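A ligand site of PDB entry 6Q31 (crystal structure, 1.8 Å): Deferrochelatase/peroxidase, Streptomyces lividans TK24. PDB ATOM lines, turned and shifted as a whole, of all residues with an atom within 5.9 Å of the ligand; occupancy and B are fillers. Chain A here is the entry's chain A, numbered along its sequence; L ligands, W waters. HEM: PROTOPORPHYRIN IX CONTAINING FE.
The backbone carbonyl oxygen of Arg 188 sits at hydrogen-bond distance from the guanidinium group of Arg 288, 3.1 Å away.
The guanidinium group of Arg 188 sits at hydrogen-bond distance from a ring nitrogen (NE2) of His 277 (3.3 Å).
The side-chain amide oxygen of Asn 189 is in hydrogen-bond range of the backbone NH of Arg 288 (2.8 Å).
The backbone carbonyl oxygen of Phe 243 is in hydrogen-bond range of the backbone NH of Val 273, at 3.1 Å.
The side-chain amide nitrogen of Asn 179 sits at hydrogen-bond distance from the side-chain carboxylate of Asp 185, 2.7 Å away.
The backbone NH (N) of Phe 183 sits at hydrogen-bond distance from the side-chain amide oxygen (OD1) of Asn 179, at 3.4 Å.
The side-chain amide oxygen of Asn 179 is in hydrogen-bond range of the backbone NH of Leu 181.
N of Leu 307 sits at hydrogen-bond distance from O of Ile 224 (2.9 Å).
NE2 of His 272 is bound to FE of the ligand, at 2.3 Å.
N of Gly 186 lies within hydrogen-bond range of O2A of the ligand (2.7 Å).
The backbone NH (N) of Arg 188 lies within hydrogen-bond range of an oxygen (O1A) of the ligand (3.1 Å).
O1D of the ligand lies within salt-bridge range of NE of Arg 188, at 2.8 Å.
NH2 of Arg 288 lies within salt-bridge range of O2A of the ligand, at 2.9 Å.
O2A of the ligand lies within hydrogen-bond range of N of Thr 187, 3.3 Å away.
Water W1 bridges O2D of the ligand (2.7 Å) and O of Arg 188 (2.9 Å).
Water W3 lies within hydrogen-bond range of the guanidinium group (NH2) of Arg 245 and an oxygen (O1A) of the ligand.
ND2 of Asn 179 touches CMB of the ligand, 3.6 Å away.
Leu 181 touches the ligand.
Phe 183 touches the ligand.
Lys 184 touches the ligand.
OD2 of Asp 185 touches CHB of the ligand (3.6 Å).
CE of Met 226 touches CBB of the ligand (3.6 Å).
CE1 of Phe 243 touches CHB of the ligand (3.5 Å).
Arg 245 touches the ligand.
CG1 of Val 273 touches O1D of the ligand (3.9 Å).
Ala 276 touches the ligand (O to CMD, 3.5 Å).
His 277 touches the ligand (CD2 to O1D, 3.4 Å).
Pro 278 touches the ligand.
Leu 307 touches the ligand (CD1 to CBB, 3.9 Å).
CZ of Phe 309 touches C3C of the ligand (3.5 Å).
CE1 of Phe 320 touches CBC of the ligand, 3.3 Å away.
Val 323 touches the ligand (CG1 to CAC, 3.9 Å).
OE1 of Gln 324 touches CBC of the ligand, at 3.6 Å.
CD1 of Leu 327 touches C3C of the ligand, 3.9 Å away.
Leu 332 touches the ligand.
Ile 336 touches the ligand (CG2 to CBB, 3.9 Å).
Hydrophobic or aromatic side chains that line the ligand: Leu 181, Phe 183, Met 226, Phe 243, His 272, Val 273, Ala 276, His 277, Pro 278, Leu 307, Phe 309, Phe 320, Val 323, Leu 327, Leu 332 and Ile 336.
25 residues have an atom within 4 Å of the ligand: Asn 179, Leu 181, Phe 183, Lys 184, Asp 185, Gly 186, Thr 187, Arg 188, Met 226, Phe 243, Arg 245, His 272, Val 273, Ala 276, His 277, Pro 278, Arg 288, Leu 307, Phe 309, Phe 320, Val 323, Gln 324, Leu 327, Leu 332 and Ile 336.
The nearest printed residue that does not touch the ligand is Leu 286 (4.03 Å).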
ATOM      1  N   ASN A 179       9.339  -2.011  14.533  1.00  0.00           N
ATOM      2  CA  ASN A 179       9.791  -3.138  15.325  1.00  0.00           C
ATOM      3  C   ASN A 179       9.819  -4.394  14.450  1.00  0.00           C
ATOM      4  O   ASN A 179       9.515  -4.370  13.251  1.00  0.00           O
ATOM      5  CB  ASN A 179       8.910  -3.302  16.572  1.00  0.00           C
ATOM      6  CG  ASN A 179       7.417  -3.349  16.252  1.00  0.00           C
ATOM      7  OD1 ASN A 179       6.990  -4.054  15.339  1.00  0.00           O
ATOM      8  ND2 ASN A 179       6.627  -2.585  16.995  1.00  0.00           N
ATOM      9  N   LEU A 181       7.878  -6.900  14.473  1.00  0.00           N
ATOM     10  CA  LEU A 181       6.571  -7.259  13.929  1.00  0.00           C
ATOM     11  C   LEU A 181       6.233  -6.474  12.674  1.00  0.00           C
ATOM     12  O   LEU A 181       5.194  -6.734  12.064  1.00  0.00           O
ATOM     13  CB  LEU A 181       5.485  -7.055  14.982  1.00  0.00           C
ATOM     14  CG  LEU A 181       5.708  -7.828  16.270  1.00  0.00           C
ATOM     15  CD1 LEU A 181       4.506  -7.726  17.195  1.00  0.00           C
ATOM     16  CD2 LEU A 181       6.039  -9.285  15.966  1.00  0.00           C
ATOM     17  N   PHE A 183       5.613  -3.118  12.369  1.00  0.00           N
ATOM     18  CA  PHE A 183       4.830  -1.914  12.594  1.00  0.00           C
ATOM     19  C   PHE A 183       5.698  -0.763  13.080  1.00  0.00           C
ATOM     20  O   PHE A 183       6.635  -0.979  13.854  1.00  0.00           O
ATOM     21  CB  PHE A 183       3.706  -2.178  13.602  1.00  0.00           C
ATOM     22  CG  PHE A 183       2.519  -2.851  13.006  1.00  0.00           C
ATOM     23  CD1 PHE A 183       2.568  -4.203  12.683  1.00  0.00           C
ATOM     24  CD2 PHE A 183       1.358  -2.152  12.749  1.00  0.00           C
ATOM     25  CE1 PHE A 183       1.493  -4.830  12.112  1.00  0.00           C
ATOM     26  CE2 PHE A 183       0.261  -2.790  12.180  1.00  0.00           C
ATOM     27  CZ  PHE A 183       0.331  -4.122  11.851  1.00  0.00           C
ATOM     28  N   LYS A 184       5.384   0.450  12.625  1.00  0.00           N
ATOM     29  CA  LYS A 184       6.020   1.643  13.169  1.00  0.00           C
ATOM     30  C   LYS A 184       5.788   1.682  14.667  1.00  0.00           C
ATOM     31  O   LYS A 184       4.728   1.297  15.171  1.00  0.00           O
ATOM     32  CB  LYS A 184       5.469   2.917  12.518  1.00  0.00           C
ATOM     33  CG  LYS A 184       5.764   3.072  11.059  1.00  0.00           C
ATOM     34  CD  LYS A 184       4.895   4.152  10.434  1.00  0.00           C
ATOM     35  CE  LYS A 184       5.400   4.532   9.053  1.00  0.00           C
ATOM     36  NZ  LYS A 184       4.517   5.560   8.409  1.00  0.00           N
ATOM     37  N   ASP A 185       6.790   2.145  15.392  1.00  0.00           N
ATOM     38  CA  ASP A 185       6.758   2.105  16.851  1.00  0.00           C
ATOM     39  C   ASP A 185       7.320   3.437  17.317  1.00  0.00           C
ATOM     40  O   ASP A 185       8.492   3.709  17.098  1.00  0.00           O
ATOM     41  CB  ASP A 185       7.590   0.938  17.378  1.00  0.00           C
ATOM     42  CG  ASP A 185       7.090   0.368  18.700  1.00  0.00           C
ATOM     43  OD1 ASP A 185       6.492   1.093  19.543  1.00  0.00           O
ATOM     44  OD2 ASP A 185       7.313  -0.835  18.907  1.00  0.00           O
ATOM     45  N   GLY A 186       6.472   4.267  17.939  1.00  0.00           N
ATOM     46  CA  GLY A 186       6.925   5.541  18.479  1.00  0.00           C
ATOM     47  C   GLY A 186       6.115   6.753  18.051  1.00  0.00           C
ATOM     48  O   GLY A 186       6.386   7.875  18.479  1.00  0.00           O
ATOM     49  N   THR A 187       5.089   6.531  17.229  1.00  0.00           N
ATOM     50  CA  THR A 187       4.292   7.635  16.704  1.00  0.00           C
ATOM     51  C   THR A 187       3.777   8.555  17.812  1.00  0.00           C
ATOM     52  O   THR A 187       4.121   9.733  17.864  1.00  0.00           O
ATOM     53  CB  THR A 187       3.138   7.047  15.877  1.00  0.00           C
ATOM     54  OG1 THR A 187       3.705   6.162  14.896  1.00  0.00           O
ATOM     55  CG2 THR A 187       2.305   8.137  15.172  1.00  0.00           C
ATOM     56  N   ARG A 188       2.984   8.014  18.741  1.00  0.00           N
ATOM     57  CA  ARG A 188       2.437   8.816  19.834  1.00  0.00           C
ATOM     58  C   ARG A 188       3.230   8.543  21.109  1.00  0.00           C
ATOM     59  O   ARG A 188       2.794   7.868  22.038  1.00  0.00           O
ATOM     60  CB  ARG A 188       0.936   8.539  20.010  1.00  0.00           C
ATOM     61  CG  ARG A 188       0.058   9.294  18.991  1.00  0.00           C
ATOM     62  CD  ARG A 188      -1.457   9.094  19.245  1.00  0.00           C
ATOM     63  NE  ARG A 188      -1.741   9.024  20.673  1.00  0.00           N
ATOM     64  CZ  ARG A 188      -1.860  10.087  21.462  1.00  0.00           C
ATOM     65  NH1 ARG A 188      -2.085   9.930  22.763  1.00  0.00           N
ATOM     66  NH2 ARG A 188      -1.772  11.310  20.958  1.00  0.00           N
ATOM     67  N   ASN A 189       4.433   9.095  21.128  1.00  0.00           N
ATOM     68  CA  ASN A 189       5.295   9.080  22.293  1.00  0.00           C
ATOM     69  C   ASN A 189       5.338  10.509  22.859  1.00  0.00           C
ATOM     70  O   ASN A 189       4.451  11.322  22.574  1.00  0.00           O
ATOM     71  CB  ASN A 189       6.665   8.527  21.898  1.00  0.00           C
ATOM     72  CG  ASN A 189       7.433   7.997  23.087  1.00  0.00           C
ATOM     73  OD1 ASN A 189       6.855   7.452  24.019  1.00  0.00           O
ATOM     74  ND2 ASN A 189       8.749   8.132  23.044  1.00  0.00           N
ATOM     75  N   ILE A 224      10.956  -8.584  26.437  1.00  0.00           N
ATOM     76  CA  ILE A 224       9.728  -9.176  25.904  1.00  0.00           C
ATOM     77  C   ILE A 224      10.062 -10.027  24.690  1.00  0.00           C
ATOM     78  O   ILE A 224      10.465  -9.494  23.639  1.00  0.00           O
ATOM     79  CB  ILE A 224       8.679  -8.112  25.552  1.00  0.00           C
ATOM     80  CG1 ILE A 224       8.415  -7.217  26.763  1.00  0.00           C
ATOM     81  CG2 ILE A 224       7.379  -8.776  25.083  1.00  0.00           C
ATOM     82  CD1 ILE A 224       7.572  -5.943  26.429  1.00  0.00           C
ATOM     83  N   MET A 226       9.103 -12.174  21.413  1.00  0.00           N
ATOM     84  CA  MET A 226       8.077 -12.206  20.376  1.00  0.00           C
ATOM     85  C   MET A 226       7.968 -13.610  19.768  1.00  0.00           C
ATOM     86  O   MET A 226       8.982 -14.253  19.462  1.00  0.00           O
ATOM     87  CB  MET A 226       8.385 -11.206  19.274  1.00  0.00           C
ATOM     88  CG  MET A 226       8.381  -9.769  19.740  1.00  0.00           C
ATOM     89  SD  MET A 226       9.074  -8.704  18.465  1.00  0.00           S
ATOM     90  CE  MET A 226       8.599  -7.102  19.108  1.00  0.00           C
ATOM     91  N   PHE A 243      -3.346  -4.238  16.462  1.00  0.00           N
ATOM     92  CA  PHE A 243      -2.805  -2.947  16.886  1.00  0.00           C
ATOM     93  C   PHE A 243      -3.834  -1.819  16.827  1.00  0.00           C
ATOM     94  O   PHE A 243      -3.836  -0.960  17.716  1.00  0.00           O
ATOM     95  CB  PHE A 243      -1.590  -2.582  16.028  1.00  0.00           C
ATOM     96  CG  PHE A 243      -0.360  -3.295  16.473  1.00  0.00           C
ATOM     97  CD1 PHE A 243       0.194  -3.022  17.714  1.00  0.00           C
ATOM     98  CD2 PHE A 243       0.221  -4.263  15.676  1.00  0.00           C
ATOM     99  CE1 PHE A 243       1.333  -3.704  18.161  1.00  0.00           C
ATOM    100  CE2 PHE A 243       1.343  -4.960  16.114  1.00  0.00           C
ATOM    101  CZ  PHE A 243       1.910  -4.675  17.356  1.00  0.00           C
ATOM    102  N   ARG A 245      -3.832   0.044  13.950  1.00  0.00           N
ATOM    103  CA  ARG A 245      -3.235   0.860  12.911  1.00  0.00           C
ATOM    104  C   ARG A 245      -2.954  -0.028  11.714  1.00  0.00           C
ATOM    105  O   ARG A 245      -2.785  -1.245  11.868  1.00  0.00           O
ATOM    106  CB  ARG A 245      -1.946   1.534  13.404  1.00  0.00           C
ATOM    107  CG  ARG A 245      -2.122   2.590  14.504  1.00  0.00           C
ATOM    108  CD  ARG A 245      -0.792   3.208  14.840  1.00  0.00           C
ATOM    109  NE  ARG A 245      -0.890   4.245  15.868  1.00  0.00           N
ATOM    110  CZ  ARG A 245      -1.043   5.547  15.609  1.00  0.00           C
ATOM    111  NH1 ARG A 245      -1.119   5.969  14.356  1.00  0.00           N
ATOM    112  NH2 ARG A 245      -1.121   6.419  16.608  1.00  0.00           N
ATOM    113  N   PRO A 262      -5.861   8.976  16.485  1.00  0.00           N
ATOM    114  CA  PRO A 262      -6.683   7.776  16.485  1.00  0.00           C
ATOM    115  C   PRO A 262      -8.097   8.090  16.935  1.00  0.00           C
ATOM    116  O   PRO A 262      -8.329   8.956  17.780  1.00  0.00           O
ATOM    117  CB  PRO A 262      -5.963   6.836  17.465  1.00  0.00           C
ATOM    118  CG  PRO A 262      -5.135   7.720  18.289  1.00  0.00           C
ATOM    119  CD  PRO A 262      -4.757   8.903  17.452  1.00  0.00           C
ATOM    120  N   HIS A 272      -4.343  -2.998  20.773  1.00  0.00           N
ATOM    121  CA  HIS A 272      -3.252  -2.533  21.623  1.00  0.00           C
ATOM    122  C   HIS A 272      -3.295  -1.021  21.812  1.00  0.00           C
ATOM    123  O   HIS A 272      -3.194  -0.535  22.942  1.00  0.00           O
ATOM    124  CB  HIS A 272      -1.940  -2.987  21.009  1.00  0.00           C
ATOM    125  CG  HIS A 272      -0.746  -2.641  21.831  1.00  0.00           C
ATOM    126  ND1 HIS A 272      -0.430  -3.317  22.988  1.00  0.00           N
ATOM    127  CD2 HIS A 272       0.205  -1.696  21.666  1.00  0.00           C
ATOM    128  CE1 HIS A 272       0.673  -2.801  23.503  1.00  0.00           C
ATOM    129  NE2 HIS A 272       1.077  -1.813  22.719  1.00  0.00           N
ATOM    130  N   VAL A 273      -3.465  -0.255  20.728  1.00  0.00           N
ATOM    131  CA  VAL A 273      -3.485   1.206  20.825  1.00  0.00           C
ATOM    132  C   VAL A 273      -4.656   1.667  21.670  1.00  0.00           C
ATOM    133  O   VAL A 273      -4.531   2.553  22.515  1.00  0.00           O
ATOM    134  CB  VAL A 273      -3.535   1.826  19.424  1.00  0.00           C
ATOM    135  CG1 VAL A 273      -3.790   3.303  19.521  1.00  0.00           C
ATOM    136  CG2 VAL A 273      -2.235   1.547  18.713  1.00  0.00           C
ATOM    137  N   ALA A 276      -3.827   1.013  25.317  1.00  0.00           N
ATOM    138  CA  ALA A 276      -2.649   1.703  25.827  1.00  0.00           C
ATOM    139  C   ALA A 276      -2.805   3.218  25.829  1.00  0.00           C
ATOM    140  O   ALA A 276      -2.022   3.899  26.492  1.00  0.00           O
ATOM    141  CB  ALA A 276      -1.420   1.334  24.987  1.00  0.00           C
ATOM    142  N   HIS A 277      -3.805   3.735  25.147  1.00  0.00           N
ATOM    143  CA  HIS A 277      -3.956   5.167  24.936  1.00  0.00           C
ATOM    144  C   HIS A 277      -4.200   5.885  26.265  1.00  0.00           C
ATOM    145  O   HIS A 277      -4.918   5.370  27.126  1.00  0.00           O
ATOM    146  CB  HIS A 277      -5.132   5.395  23.977  1.00  0.00           C
ATOM    147  CG  HIS A 277      -5.176   6.770  23.379  1.00  0.00           C
ATOM    148  ND1 HIS A 277      -5.766   7.846  24.026  1.00  0.00           N
ATOM    149  CD2 HIS A 277      -4.699   7.249  22.202  1.00  0.00           C
ATOM    150  CE1 HIS A 277      -5.655   8.913  23.263  1.00  0.00           C
ATOM    151  NE2 HIS A 277      -5.016   8.585  22.154  1.00  0.00           N
ATOM    152  N   PRO A 278      -3.603   7.063  26.478  1.00  0.00           N
ATOM    153  CA  PRO A 278      -3.839   7.795  27.739  1.00  0.00           C
ATOM    154  C   PRO A 278      -5.318   7.930  28.109  1.00  0.00           C
ATOM    155  O   PRO A 278      -5.664   7.839  29.291  1.00  0.00           O
ATOM    156  CB  PRO A 278      -3.191   9.157  27.471  1.00  0.00           C
ATOM    157  CG  PRO A 278      -2.073   8.855  26.542  1.00  0.00           C
ATOM    158  CD  PRO A 278      -2.509   7.657  25.701  1.00  0.00           C
ATOM    159  N   LEU A 286       3.403   7.712  28.978  1.00  0.00           N
ATOM    160  CA  LEU A 286       4.737   7.138  29.162  1.00  0.00           C
ATOM    161  C   LEU A 286       5.688   7.682  28.103  1.00  0.00           C
ATOM    162  O   LEU A 286       5.266   8.015  26.994  1.00  0.00           O
ATOM    163  CB  LEU A 286       4.709   5.603  29.049  1.00  0.00           C
ATOM    164  CG  LEU A 286       3.749   4.861  29.953  1.00  0.00           C
ATOM    165  CD1 LEU A 286       3.803   3.381  29.662  1.00  0.00           C
ATOM    166  CD2 LEU A 286       4.122   5.151  31.394  1.00  0.00           C
ATOM    167  N   ARG A 288       8.359   6.098  25.954  1.00  0.00           N
ATOM    168  CA  ARG A 288       8.858   4.815  25.488  1.00  0.00           C
ATOM    169  C   ARG A 288      10.199   5.005  24.772  1.00  0.00           C
ATOM    170  O   ARG A 288      10.336   5.910  23.940  1.00  0.00           O
ATOM    171  CB  ARG A 288       7.827   4.171  24.550  1.00  0.00           C
ATOM    172  CG  ARG A 288       6.678   3.468  25.306  1.00  0.00           C
ATOM    173  CD  ARG A 288       5.557   2.982  24.385  1.00  0.00           C
ATOM    174  NE  ARG A 288       4.983   4.085  23.621  1.00  0.00           N
ATOM    175  CZ  ARG A 288       4.782   4.083  22.306  1.00  0.00           C
ATOM    176  NH1 ARG A 288       5.095   3.009  21.579  1.00  0.00           N
ATOM    177  NH2 ARG A 288       4.251   5.158  21.724  1.00  0.00           N
ATOM    178  N   LEU A 307      11.672  -7.493  21.980  1.00  0.00           N
ATOM    179  CA  LEU A 307      11.745  -6.047  22.160  1.00  0.00           C
ATOM    180  C   LEU A 307      12.197  -5.772  23.586  1.00  0.00           C
ATOM    181  O   LEU A 307      11.613  -6.312  24.530  1.00  0.00           O
ATOM    182  CB  LEU A 307      10.380  -5.390  21.893  1.00  0.00           C
ATOM    183  CG  LEU A 307      10.296  -3.871  21.826  1.00  0.00           C
ATOM    184  CD1 LEU A 307       9.081  -3.442  21.006  1.00  0.00           C
ATOM    185  CD2 LEU A 307      10.216  -3.288  23.214  1.00  0.00           C
ATOM    186  N   PHE A 309      11.996  -3.397  26.180  1.00  0.00           N
ATOM    187  CA  PHE A 309      11.094  -2.284  26.379  1.00  0.00           C
ATOM    188  C   PHE A 309      11.566  -1.419  27.555  1.00  0.00           C
ATOM    189  O   PHE A 309      11.847  -1.939  28.645  1.00  0.00           O
ATOM    190  CB  PHE A 309       9.678  -2.827  26.591  1.00  0.00           C
ATOM    191  CG  PHE A 309       8.644  -1.774  26.863  1.00  0.00           C
ATOM    192  CD1 PHE A 309       8.378  -1.373  28.166  1.00  0.00           C
ATOM    193  CD2 PHE A 309       7.922  -1.213  25.816  1.00  0.00           C
ATOM    194  CE1 PHE A 309       7.413  -0.411  28.425  1.00  0.00           C
ATOM    195  CE2 PHE A 309       6.956  -0.232  26.067  1.00  0.00           C
ATOM    196  CZ  PHE A 309       6.704   0.162  27.380  1.00  0.00           C
ATOM    197  N   PHE A 320       3.620   3.148  34.280  1.00  0.00           N
ATOM    198  CA  PHE A 320       3.690   1.822  33.689  1.00  0.00           C
ATOM    199  C   PHE A 320       2.638   0.882  34.273  1.00  0.00           C
ATOM    200  O   PHE A 320       2.060   0.060  33.550  1.00  0.00           O
ATOM    201  CB  PHE A 320       5.081   1.222  33.860  1.00  0.00           C
ATOM    202  CG  PHE A 320       5.179  -0.170  33.369  1.00  0.00           C
ATOM    203  CD1 PHE A 320       5.364  -0.436  32.028  1.00  0.00           C
ATOM    204  CD2 PHE A 320       5.073  -1.226  34.255  1.00  0.00           C
ATOM    205  CE1 PHE A 320       5.441  -1.739  31.565  1.00  0.00           C
ATOM    206  CE2 PHE A 320       5.154  -2.517  33.796  1.00  0.00           C
ATOM    207  CZ  PHE A 320       5.333  -2.777  32.468  1.00  0.00           C
ATOM    208  N   VAL A 323      -1.157   1.288  32.924  1.00  0.00           N
ATOM    209  CA  VAL A 323      -1.205   0.931  31.513  1.00  0.00           C
ATOM    210  C   VAL A 323      -1.019  -0.575  31.329  1.00  0.00           C
ATOM    211  O   VAL A 323      -1.796  -1.234  30.642  1.00  0.00           O
ATOM    212  CB  VAL A 323      -0.183   1.753  30.688  1.00  0.00           C
ATOM    213  CG1 VAL A 323      -0.318   1.419  29.210  1.00  0.00           C
ATOM    214  CG2 VAL A 323      -0.407   3.273  30.881  1.00  0.00           C
ATOM    215  N   GLN A 324       0.011  -1.154  31.967  1.00  0.00           N
ATOM    216  CA  GLN A 324       0.209  -2.591  31.818  1.00  0.00           C
ATOM    217  C   GLN A 324      -0.960  -3.386  32.412  1.00  0.00           C
ATOM    218  O   GLN A 324      -1.336  -4.437  31.879  1.00  0.00           O
ATOM    219  CB  GLN A 324       1.554  -3.008  32.434  1.00  0.00           C
ATOM    220  CG  GLN A 324       1.846  -4.520  32.478  1.00  0.00           C
ATOM    221  CD  GLN A 324       2.063  -5.170  31.107  1.00  0.00           C
ATOM    222  OE1 GLN A 324       2.417  -4.514  30.140  1.00  0.00           O
ATOM    223  NE2 GLN A 324       1.861  -6.468  31.047  1.00  0.00           N
ATOM    224  N   LEU A 327      -3.521  -3.747  29.891  1.00  0.00           N
ATOM    225  CA  LEU A 327      -3.201  -4.624  28.766  1.00  0.00           C
ATOM    226  C   LEU A 327      -3.486  -6.094  29.066  1.00  0.00           C
ATOM    227  O   LEU A 327      -3.074  -6.966  28.299  1.00  0.00           O
ATOM    228  CB  LEU A 327      -1.741  -4.444  28.344  1.00  0.00           C
ATOM    229  CG  LEU A 327      -1.316  -3.012  28.000  1.00  0.00           C
ATOM    230  CD1 LEU A 327       0.145  -2.939  27.533  1.00  0.00           C
ATOM    231  CD2 LEU A 327      -2.252  -2.397  26.964  1.00  0.00           C
ATOM    232  N   LEU A 332      -2.423  -8.272  21.585  1.00  0.00           N
ATOM    233  CA  LEU A 332      -1.006  -8.533  21.381  1.00  0.00           C
ATOM    234  C   LEU A 332      -0.478  -9.642  22.286  1.00  0.00           C
ATOM    235  O   LEU A 332       0.557 -10.247  21.966  1.00  0.00           O
ATOM    236  CB  LEU A 332      -0.209  -7.248  21.602  1.00  0.00           C
ATOM    237  CG  LEU A 332       1.283  -7.243  21.328  1.00  0.00           C
ATOM    238  CD1 LEU A 332       1.527  -7.642  19.879  1.00  0.00           C
ATOM    239  CD2 LEU A 332       1.842  -5.857  21.594  1.00  0.00           C
ATOM    240  N   ILE A 336       3.425 -12.375  22.451  1.00  0.00           N
ATOM    241  CA  ILE A 336       4.567 -11.870  23.190  1.00  0.00           C
ATOM    242  C   ILE A 336       4.583 -12.511  24.568  1.00  0.00           C
ATOM    243  O   ILE A 336       3.581 -13.057  25.025  1.00  0.00           O
ATOM    244  CB  ILE A 336       4.571 -10.327  23.322  1.00  0.00           C
ATOM    245  CG1 ILE A 336       3.329  -9.859  24.088  1.00  0.00           C
ATOM    246  CG2 ILE A 336       4.608  -9.676  21.940  1.00  0.00           C
ATOM    247  CD1 ILE A 336       3.460  -8.463  24.702  1.00  0.00           C
ATOM    248  N   HIS A 338       6.545 -11.563  28.466  1.00  0.00           N
ATOM    249  CA  HIS A 338       7.516 -10.827  29.269  1.00  0.00           C
ATOM    250  C   HIS A 338       8.373 -11.836  30.034  1.00  0.00           C
ATOM    251  O   HIS A 338       7.841 -12.726  30.699  1.00  0.00           O
ATOM    252  CB  HIS A 338       6.812  -9.895  30.266  1.00  0.00           C
ATOM    253  CG  HIS A 338       6.010  -8.811  29.621  1.00  0.00           C
ATOM    254  ND1 HIS A 338       6.239  -7.470  29.852  1.00  0.00           N
ATOM    255  CD2 HIS A 338       4.969  -8.867  28.755  1.00  0.00           C
ATOM    256  CE1 HIS A 338       5.389  -6.749  29.155  1.00  0.00           C
ATOM    257  NE2 HIS A 338       4.602  -7.569  28.473  1.00  0.00           N
HETATM  258  CHA HEM L   1       1.716   2.197  20.842  1.00  0.00           C
HETATM  259  CHB HEM L   1       3.930  -1.957  19.632  1.00  0.00           C
HETATM  260  CHC HEM L   1       4.498  -3.141  24.303  1.00  0.00           C
HETATM  261  CHD HEM L   1       2.449   1.079  25.529  1.00  0.00           C
HETATM  262  C1A HEM L   1       2.243   1.173  20.094  1.00  0.00           C
HETATM  263  C2A HEM L   1       2.206   1.054  18.653  1.00  0.00           C
HETATM  264  C3A HEM L   1       2.813  -0.113  18.347  1.00  0.00           C
HETATM  265  C4A HEM L   1       3.249  -0.753  19.553  1.00  0.00           C
HETATM  266  CMA HEM L   1       3.043  -0.732  16.944  1.00  0.00           C
HETATM  267  CAA HEM L   1       1.560   2.082  17.695  1.00  0.00           C
HETATM  268  CBA HEM L   1       2.502   3.267  17.331  1.00  0.00           C
HETATM  269  CGA HEM L   1       2.883   4.192  18.472  1.00  0.00           C
HETATM  270  O1A HEM L   1       2.082   5.097  18.815  1.00  0.00           O
HETATM  271  O2A HEM L   1       3.986   4.050  19.058  1.00  0.00           O
HETATM  272  C1B HEM L   1       4.297  -2.626  20.775  1.00  0.00           C
HETATM  273  C2B HEM L   1       4.974  -3.902  20.841  1.00  0.00           C
HETATM  274  C3B HEM L   1       5.118  -4.239  22.132  1.00  0.00           C
HETATM  275  C4B HEM L   1       4.547  -3.187  22.923  1.00  0.00           C
HETATM  276  CMB HEM L   1       5.436  -4.685  19.600  1.00  0.00           C
HETATM  277  CAB HEM L   1       5.821  -5.493  22.720  1.00  0.00           C
HETATM  278  CBB HEM L   1       6.578  -6.270  21.949  1.00  0.00           C
HETATM  279  C1C HEM L   1       3.985  -2.096  25.024  1.00  0.00           C
HETATM  280  C2C HEM L   1       3.918  -2.044  26.469  1.00  0.00           C
HETATM  281  C3C HEM L   1       3.357  -0.861  26.807  1.00  0.00           C
HETATM  282  C4C HEM L   1       3.047  -0.153  25.598  1.00  0.00           C
HETATM  283  CMC HEM L   1       4.473  -3.187  27.342  1.00  0.00           C
HETATM  284  CAC HEM L   1       3.040  -0.293  28.199  1.00  0.00           C
HETATM  285  CBC HEM L   1       3.096  -1.056  29.295  1.00  0.00           C
HETATM  286  C1D HEM L   1       2.120   1.752  24.368  1.00  0.00           C
HETATM  287  C2D HEM L   1       1.605   3.090  24.310  1.00  0.00           C
HETATM  288  C3D HEM L   1       1.392   3.414  23.043  1.00  0.00           C
HETATM  289  C4D HEM L   1       1.768   2.278  22.221  1.00  0.00           C
HETATM  290  CMD HEM L   1       1.340   3.957  25.558  1.00  0.00           C
HETATM  291  CAD HEM L   1       0.837   4.758  22.528  1.00  0.00           C
HETATM  292  CBD HEM L   1      -0.665   4.633  22.329  1.00  0.00           C
HETATM  293  CGD HEM L   1      -1.213   6.007  22.081  1.00  0.00           C
HETATM  294  O1D HEM L   1      -1.728   6.245  20.959  1.00  0.00           O
HETATM  295  O2D HEM L   1      -1.090   6.865  22.987  1.00  0.00           O
HETATM  296  NA  HEM L   1       2.871   0.049  20.608  1.00  0.00           N
HETATM  297  NB  HEM L   1       4.033  -2.226  22.055  1.00  0.00           N
HETATM  298  NC  HEM L   1       3.431  -0.942  24.523  1.00  0.00           N
HETATM  299  ND  HEM L   1       2.208   1.296  23.072  1.00  0.00           N
HETATM  300 FE   HEM L   1       2.981  -0.533  22.590  1.00  0.00          FE
HETATM  301  O   HOH W   1       0.916   8.128  24.235  1.00  0.00           O
HETATM  302  O   HOH W   2       1.749   7.131  26.549  1.00  0.00           O
HETATM  303  O   HOH W   3      -0.664   5.032  18.576  1.00  0.00           O
